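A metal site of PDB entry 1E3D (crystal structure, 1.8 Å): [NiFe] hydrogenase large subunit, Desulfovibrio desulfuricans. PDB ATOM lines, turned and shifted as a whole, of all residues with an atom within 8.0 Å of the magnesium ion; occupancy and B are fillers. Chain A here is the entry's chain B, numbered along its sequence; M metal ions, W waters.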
ATOM      1  N   PHE A  48       2.313 -10.538  10.502  1.00  0.00           N
ATOM      2  CA  PHE A  48       2.706 -11.768   9.835  1.00  0.00           C
ATOM      3  C   PHE A  48       4.202 -11.659   9.448  1.00  0.00           C
ATOM      4  O   PHE A  48       4.643 -10.572   9.111  1.00  0.00           O
ATOM      5  CB  PHE A  48       1.849 -12.072   8.620  1.00  0.00           C
ATOM      6  CG  PHE A  48       2.158 -13.265   7.751  1.00  0.00           C
ATOM      7  CD1 PHE A  48       1.746 -14.535   8.112  1.00  0.00           C
ATOM      8  CD2 PHE A  48       2.860 -13.119   6.560  1.00  0.00           C
ATOM      9  CE1 PHE A  48       2.027 -15.632   7.327  1.00  0.00           C
ATOM     10  CE2 PHE A  48       3.121 -14.212   5.773  1.00  0.00           C
ATOM     11  CZ  PHE A  48       2.738 -15.485   6.147  1.00  0.00           C
ATOM     12  N   GLU A  52       6.933 -20.440   7.999  1.00  0.00           N
ATOM     13  CA  GLU A  52       6.713 -21.686   7.262  1.00  0.00           C
ATOM     14  C   GLU A  52       7.220 -21.607   5.823  1.00  0.00           C
ATOM     15  O   GLU A  52       7.901 -22.525   5.333  1.00  0.00           O
ATOM     16  CB  GLU A  52       5.218 -22.046   7.307  1.00  0.00           C
ATOM     17  CG  GLU A  52       4.771 -22.474   8.708  1.00  0.00           C
ATOM     18  CD  GLU A  52       3.302 -22.237   8.980  1.00  0.00           C
ATOM     19  OE1 GLU A  52       2.712 -21.367   8.296  1.00  0.00           O
ATOM     20  OE2 GLU A  52       2.761 -22.905   9.886  1.00  0.00           O
ATOM     21  N   GLU A 329      -6.771 -26.843  10.376  1.00  0.00           N
ATOM     22  CA  GLU A 329      -6.755 -25.392  10.541  1.00  0.00           C
ATOM     23  C   GLU A 329      -7.658 -24.688   9.540  1.00  0.00           C
ATOM     24  O   GLU A 329      -7.454 -24.753   8.333  1.00  0.00           O
ATOM     25  CB  GLU A 329      -5.319 -24.859  10.451  1.00  0.00           C
ATOM     26  CG  GLU A 329      -4.383 -25.310  11.575  1.00  0.00           C
ATOM     27  CD  GLU A 329      -3.012 -24.664  11.448  1.00  0.00           C
ATOM     28  OE1 GLU A 329      -2.268 -25.001  10.511  1.00  0.00           O
ATOM     29  OE2 GLU A 329      -2.669 -23.798  12.274  1.00  0.00           O
ATOM     30  N   TYR A 336      -5.918 -15.654   4.964  1.00  0.00           N
ATOM     31  CA  TYR A 336      -5.252 -16.570   4.033  1.00  0.00           C
ATOM     32  C   TYR A 336      -6.275 -17.102   3.029  1.00  0.00           C
ATOM     33  O   TYR A 336      -7.476 -17.016   3.273  1.00  0.00           O
ATOM     34  CB  TYR A 336      -4.588 -17.736   4.758  1.00  0.00           C
ATOM     35  CG  TYR A 336      -3.597 -17.313   5.837  1.00  0.00           C
ATOM     36  CD1 TYR A 336      -2.295 -16.969   5.538  1.00  0.00           C
ATOM     37  CD2 TYR A 336      -4.027 -17.287   7.153  1.00  0.00           C
ATOM     38  CE1 TYR A 336      -1.411 -16.594   6.544  1.00  0.00           C
ATOM     39  CE2 TYR A 336      -3.154 -16.920   8.160  1.00  0.00           C
ATOM     40  CZ  TYR A 336      -1.862 -16.576   7.851  1.00  0.00           C
ATOM     41  OH  TYR A 336      -1.031 -16.204   8.876  1.00  0.00           O
ATOM     42  N   PRO A 343      -2.436 -30.282   8.873  1.00  0.00           N
ATOM     43  CA  PRO A 343      -1.107 -29.655   8.719  1.00  0.00           C
ATOM     44  C   PRO A 343      -0.132 -30.376   7.803  1.00  0.00           C
ATOM     45  O   PRO A 343       0.721 -29.656   7.269  1.00  0.00           O
ATOM     46  CB  PRO A 343      -0.546 -29.610  10.148  1.00  0.00           C
ATOM     47  CG  PRO A 343      -1.736 -29.777  11.035  1.00  0.00           C
ATOM     48  CD  PRO A 343      -2.694 -30.653  10.263  1.00  0.00           C
ATOM     49  N   GLY A 346      -0.771 -28.518   4.943  1.00  0.00           N
ATOM     50  CA  GLY A 346      -1.028 -27.105   5.182  1.00  0.00           C
ATOM     51  C   GLY A 346      -0.533 -26.164   4.108  1.00  0.00           C
ATOM     52  O   GLY A 346       0.370 -26.491   3.340  1.00  0.00           O
ATOM     53  N   GLU A 347      -1.143 -24.990   4.073  1.00  0.00           N
ATOM     54  CA  GLU A 347      -0.797 -23.894   3.176  1.00  0.00           C
ATOM     55  C   GLU A 347      -0.904 -22.532   3.844  1.00  0.00           C
ATOM     56  O   GLU A 347      -1.781 -22.252   4.658  1.00  0.00           O
ATOM     57  CB  GLU A 347      -1.716 -23.931   1.940  1.00  0.00           C
ATOM     58  CG  GLU A 347      -1.575 -22.673   1.091  1.00  0.00           C
ATOM     59  CD  GLU A 347      -2.667 -22.611   0.039  1.00  0.00           C
ATOM     60  OE1 GLU A 347      -2.509 -23.309  -0.988  1.00  0.00           O
ATOM     61  OE2 GLU A 347      -3.659 -21.883   0.241  1.00  0.00           O
ATOM     62  N   THR A 348       0.014 -21.623   3.496  1.00  0.00           N
ATOM     63  CA  THR A 348       0.033 -20.312   4.132  1.00  0.00           C
ATOM     64  C   THR A 348       0.227 -19.235   3.078  1.00  0.00           C
ATOM     65  O   THR A 348       1.229 -18.538   2.954  1.00  0.00           O
ATOM     66  CB  THR A 348       1.133 -20.288   5.190  1.00  0.00           C
ATOM     67  OG1 THR A 348       1.002 -21.505   5.933  1.00  0.00           O
ATOM     68  CG2 THR A 348       0.960 -19.095   6.138  1.00  0.00           C
ATOM     69  N   TRP A 363      -4.382 -12.713  11.320  1.00  0.00           N
ATOM     70  CA  TRP A 363      -3.323 -13.511  10.723  1.00  0.00           C
ATOM     71  C   TRP A 363      -3.150 -14.885  11.379  1.00  0.00           C
ATOM     72  O   TRP A 363      -2.347 -15.769  11.071  1.00  0.00           O
ATOM     73  CB  TRP A 363      -1.996 -12.744  10.788  1.00  0.00           C
ATOM     74  CG  TRP A 363      -1.869 -11.598   9.837  1.00  0.00           C
ATOM     75  CD1 TRP A 363      -1.821 -10.264  10.143  1.00  0.00           C
ATOM     76  CD2 TRP A 363      -1.761 -11.679   8.422  1.00  0.00           C
ATOM     77  NE1 TRP A 363      -1.689  -9.510   8.997  1.00  0.00           N
ATOM     78  CE2 TRP A 363      -1.653 -10.364   7.920  1.00  0.00           C
ATOM     79  CE3 TRP A 363      -1.739 -12.748   7.514  1.00  0.00           C
ATOM     80  CZ2 TRP A 363      -1.523 -10.089   6.565  1.00  0.00           C
ATOM     81  CZ3 TRP A 363      -1.617 -12.459   6.165  1.00  0.00           C
ATOM     82  CH2 TRP A 363      -1.512 -11.143   5.694  1.00  0.00           C
ATOM     83  N   LYS A 365      -4.547 -18.552  11.934  1.00  0.00           N
ATOM     84  CA  LYS A 365      -5.459 -19.588  11.464  1.00  0.00           C
ATOM     85  C   LYS A 365      -6.357 -19.985  12.619  1.00  0.00           C
ATOM     86  O   LYS A 365      -6.031 -19.732  13.788  1.00  0.00           O
ATOM     87  CB  LYS A 365      -4.692 -20.785  10.936  1.00  0.00           C
ATOM     88  CG  LYS A 365      -3.891 -20.460   9.674  1.00  0.00           C
ATOM     89  CD  LYS A 365      -3.141 -21.681   9.163  1.00  0.00           C
ATOM     90  CE  LYS A 365      -2.368 -21.400   7.871  1.00  0.00           C
ATOM     91  NZ  LYS A 365      -1.361 -22.466   7.594  1.00  0.00           N
ATOM     92  N   PRO A 367      -7.383 -23.228  14.272  1.00  0.00           N
ATOM     93  CA  PRO A 367      -7.281 -24.683  14.448  1.00  0.00           C
ATOM     94  C   PRO A 367      -8.493 -25.232  15.220  1.00  0.00           C
ATOM     95  O   PRO A 367      -8.995 -24.646  16.153  1.00  0.00           O
ATOM     96  CB  PRO A 367      -6.043 -24.911  15.315  1.00  0.00           C
ATOM     97  CG  PRO A 367      -5.403 -23.576  15.476  1.00  0.00           C
ATOM     98  CD  PRO A 367      -6.457 -22.528  15.180  1.00  0.00           C
ATOM     99  N   SER A 473       2.736 -28.168  18.008  1.00  0.00           N
ATOM    100  CA  SER A 473       3.100 -29.263  17.121  1.00  0.00           C
ATOM    101  C   SER A 473       3.734 -28.713  15.857  1.00  0.00           C
ATOM    102  O   SER A 473       3.281 -27.726  15.288  1.00  0.00           O
ATOM    103  CB  SER A 473       1.873 -30.140  16.842  1.00  0.00           C
ATOM    104  OG  SER A 473       0.817 -29.458  16.177  1.00  0.00           O
ATOM    105  N   TRP A 475       4.991 -30.017  11.980  1.00  0.00           N
ATOM    106  CA  TRP A 475       4.663 -31.034  10.981  1.00  0.00           C
ATOM    107  C   TRP A 475       5.510 -30.868   9.727  1.00  0.00           C
ATOM    108  O   TRP A 475       5.456 -29.862   9.020  1.00  0.00           O
ATOM    109  CB  TRP A 475       3.184 -30.941  10.648  1.00  0.00           C
ATOM    110  CG  TRP A 475       2.207 -30.918  11.777  1.00  0.00           C
ATOM    111  CD1 TRP A 475       1.999 -29.940  12.695  1.00  0.00           C
ATOM    112  CD2 TRP A 475       1.282 -31.956  12.123  1.00  0.00           C
ATOM    113  NE1 TRP A 475       1.004 -30.292  13.593  1.00  0.00           N
ATOM    114  CE2 TRP A 475       0.557 -31.534  13.255  1.00  0.00           C
ATOM    115  CE3 TRP A 475       0.997 -33.215  11.576  1.00  0.00           C
ATOM    116  CZ2 TRP A 475      -0.431 -32.322  13.846  1.00  0.00           C
ATOM    117  CZ3 TRP A 475       0.020 -33.990  12.185  1.00  0.00           C
ATOM    118  CH2 TRP A 475      -0.684 -33.536  13.297  1.00  0.00           C
ATOM    119  N   PHE A 486       6.482 -27.516   5.747  1.00  0.00           N
ATOM    120  CA  PHE A 486       6.692 -27.419   7.200  1.00  0.00           C
ATOM    121  C   PHE A 486       5.590 -26.551   7.775  1.00  0.00           C
ATOM    122  O   PHE A 486       5.436 -25.405   7.346  1.00  0.00           O
ATOM    123  CB  PHE A 486       8.074 -26.851   7.506  1.00  0.00           C
ATOM    124  CG  PHE A 486       8.558 -27.113   8.922  1.00  0.00           C
ATOM    125  CD1 PHE A 486       7.977 -26.484  10.006  1.00  0.00           C
ATOM    126  CD2 PHE A 486       9.592 -28.002   9.157  1.00  0.00           C
ATOM    127  CE1 PHE A 486       8.409 -26.713  11.305  1.00  0.00           C
ATOM    128  CE2 PHE A 486      10.044 -28.238  10.449  1.00  0.00           C
ATOM    129  CZ  PHE A 486       9.435 -27.606  11.520  1.00  0.00           C
ATOM    130  N   GLN A 487       4.826 -27.086   8.726  1.00  0.00           N
ATOM    131  CA  GLN A 487       3.754 -26.307   9.318  1.00  0.00           C
ATOM    132  C   GLN A 487       3.847 -26.329  10.845  1.00  0.00           C
ATOM    133  O   GLN A 487       4.034 -27.392  11.437  1.00  0.00           O
ATOM    134  CB  GLN A 487       2.399 -26.832   8.853  1.00  0.00           C
ATOM    135  CG  GLN A 487       2.171 -26.703   7.352  1.00  0.00           C
ATOM    136  CD  GLN A 487       1.894 -25.284   6.909  1.00  0.00           C
ATOM    137  OE1 GLN A 487       1.203 -24.513   7.580  1.00  0.00           O
ATOM    138  NE2 GLN A 487       2.441 -24.897   5.744  1.00  0.00           N
ATOM    139  N   LEU A 488       3.698 -25.152  11.432  1.00  0.00           N
ATOM    140  CA  LEU A 488       3.595 -25.031  12.877  1.00  0.00           C
ATOM    141  C   LEU A 488       2.130 -24.774  13.258  1.00  0.00           C
ATOM    142  O   LEU A 488       1.471 -23.962  12.610  1.00  0.00           O
ATOM    143  CB  LEU A 488       4.422 -23.908  13.464  1.00  0.00           C
ATOM    144  CG  LEU A 488       5.927 -23.854  13.262  1.00  0.00           C
ATOM    145  CD1 LEU A 488       6.303 -23.527  11.826  1.00  0.00           C
ATOM    146  CD2 LEU A 488       6.529 -22.818  14.233  1.00  0.00           C
ATOM    147  N   VAL A 489       1.663 -25.466  14.289  1.00  0.00           N
ATOM    148  CA  VAL A 489       0.360 -25.239  14.926  1.00  0.00           C
ATOM    149  C   VAL A 489       0.672 -24.999  16.402  1.00  0.00           C
ATOM    150  O   VAL A 489       1.173 -25.898  17.092  1.00  0.00           O
ATOM    151  CB  VAL A 489      -0.640 -26.378  14.683  1.00  0.00           C
ATOM    152  CG1 VAL A 489      -2.052 -25.964  15.091  1.00  0.00           C
ATOM    153  CG2 VAL A 489      -0.616 -26.814  13.226  1.00  0.00           C
ATOM    154  N   VAL A 490       0.441 -23.785  16.860  1.00  0.00           N
ATOM    155  CA  VAL A 490       1.054 -23.274  18.097  1.00  0.00           C
ATOM    156  C   VAL A 490      -0.037 -22.976  19.117  1.00  0.00           C
ATOM    157  O   VAL A 490      -1.164 -22.684  18.705  1.00  0.00           O
ATOM    158  CB  VAL A 490       1.926 -22.074  17.710  1.00  0.00           C
ATOM    159  CG1 VAL A 490       2.795 -21.533  18.832  1.00  0.00           C
ATOM    160  CG2 VAL A 490       2.855 -22.431  16.535  1.00  0.00           C
ATOM    161  N   THR A 493      -2.157 -19.991  18.653  1.00  0.00           N
ATOM    162  CA  THR A 493      -3.010 -20.207  17.485  1.00  0.00           C
ATOM    163  C   THR A 493      -4.389 -20.765  17.866  1.00  0.00           C
ATOM    164  O   THR A 493      -5.429 -20.307  17.365  1.00  0.00           O
ATOM    165  CB  THR A 493      -2.399 -21.178  16.464  1.00  0.00           C
ATOM    166  OG1 THR A 493      -1.017 -20.927  16.281  1.00  0.00           O
ATOM    167  CG2 THR A 493      -3.102 -20.934  15.130  1.00  0.00           C
ATOM    168  N   CYS A 539       4.285 -16.361  18.218  1.00  0.00           N
ATOM    169  CA  CYS A 539       3.958 -17.774  18.240  1.00  0.00           C
ATOM    170  C   CYS A 539       2.761 -18.148  17.369  1.00  0.00           C
ATOM    171  O   CYS A 539       2.857 -19.013  16.486  1.00  0.00           O
ATOM    172  CB  CYS A 539       3.674 -18.239  19.690  1.00  0.00           C
ATOM    173  SG  CYS A 539       5.101 -19.000  20.476  1.00  0.00           S
ATOM    174  N   SER A 540       1.622 -17.508  17.614  1.00  0.00           N
ATOM    175  CA  SER A 540       0.351 -17.900  17.018  1.00  0.00           C
ATOM    176  C   SER A 540       0.341 -17.722  15.509  1.00  0.00           C
ATOM    177  O   SER A 540      -0.198 -18.610  14.840  1.00  0.00           O
ATOM    178  CB  SER A 540      -0.829 -17.165  17.661  1.00  0.00           C
ATOM    179  OG  SER A 540      -0.873 -15.782  17.363  1.00  0.00           O
ATOM    180  N   THR A 541       0.934 -16.637  15.001  1.00  0.00           N
ATOM    181  CA  THR A 541       1.027 -16.375  13.575  1.00  0.00           C
ATOM    182  C   THR A 541       2.257 -16.917  12.864  1.00  0.00           C
ATOM    183  O   THR A 541       2.153 -17.447  11.746  1.00  0.00           O
ATOM    184  CB  THR A 541       1.052 -14.842  13.338  1.00  0.00           C
ATOM    185  OG1 THR A 541      -0.146 -14.246  13.856  1.00  0.00           O
ATOM    186  CG2 THR A 541       1.095 -14.613  11.826  1.00  0.00           C
ATOM    187  N   HIS A 542       3.441 -16.827  13.455  1.00  0.00           N
ATOM    188  CA  HIS A 542       4.724 -17.203  12.884  1.00  0.00           C
ATOM    189  C   HIS A 542       4.802 -16.696  11.435  1.00  0.00           C
ATOM    190  O   HIS A 542       5.226 -17.434  10.535  1.00  0.00           O
ATOM    191  CB  HIS A 542       5.025 -18.699  12.943  1.00  0.00           C
ATOM    192  CG  HIS A 542       3.851 -19.646  12.802  1.00  0.00           C
ATOM    193  ND1 HIS A 542       2.948 -19.842  13.834  1.00  0.00           N
ATOM    194  CD2 HIS A 542       3.427 -20.408  11.785  1.00  0.00           C
ATOM    195  CE1 HIS A 542       2.026 -20.703  13.435  1.00  0.00           C
ATOM    196  NE2 HIS A 542       2.280 -21.070  12.196  1.00  0.00           N
ATOM    197  OXT HIS A 542       4.403 -15.528  11.232  1.00  0.00           O
HETATM  198 MG    MG M   1       1.013 -22.507  11.114  1.00  0.00          MG
HETATM  199  O   HOH W   1      -0.153 -23.865   9.917  1.00  0.00           O
HETATM  200  O   HOH W   2      -0.733 -22.057  12.231  1.00  0.00           O
HETATM  201  O   HOH W   3       0.510 -20.849   9.690  1.00  0.00           O
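The side-chain amide oxygen (OE1) of Gln 487 lies close to the side-chain carboxylate (OE2) of Glu 52. The side-chain hydroxyl (OG1) of Thr 348 sits at hydrogen-bond distance from the side-chain carboxylate (OE1) of Glu 52. ND1 of His 542 is in hydrogen-bond range of O of Cys 539 (2.8 Å).
Of the 23 residues printed, 3 come within 4 Å of the magnesium ion. The nearest printed residue that does not touch the magnesium ion is Gln 487 (4.1 Å).
The magnesium ion is bound by water W2 (2.1 Å), O of Leu 488 (2.1 Å), water W1 (2.2 Å), OE2 of Glu 52 (2.2 Å), NE2 of His 542 (2.2 Å) and water W3 (2.2 Å). The magnesium ion has six donor atoms within binding distance.
Water W1 lies within hydrogen-bond range of the side-chain carboxylate (OE1) of Glu 329 (2.5 Å), the side-chain amide oxygen (OE1) of Gln 487 (2.8 Å) and the side-chain amino group (NZ) of Lys 365 (3.0 Å). Water W3 lies within hydrogen-bond range of the side-chain carboxylate of Glu 52 and the side-chain amino group of Lys 365.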
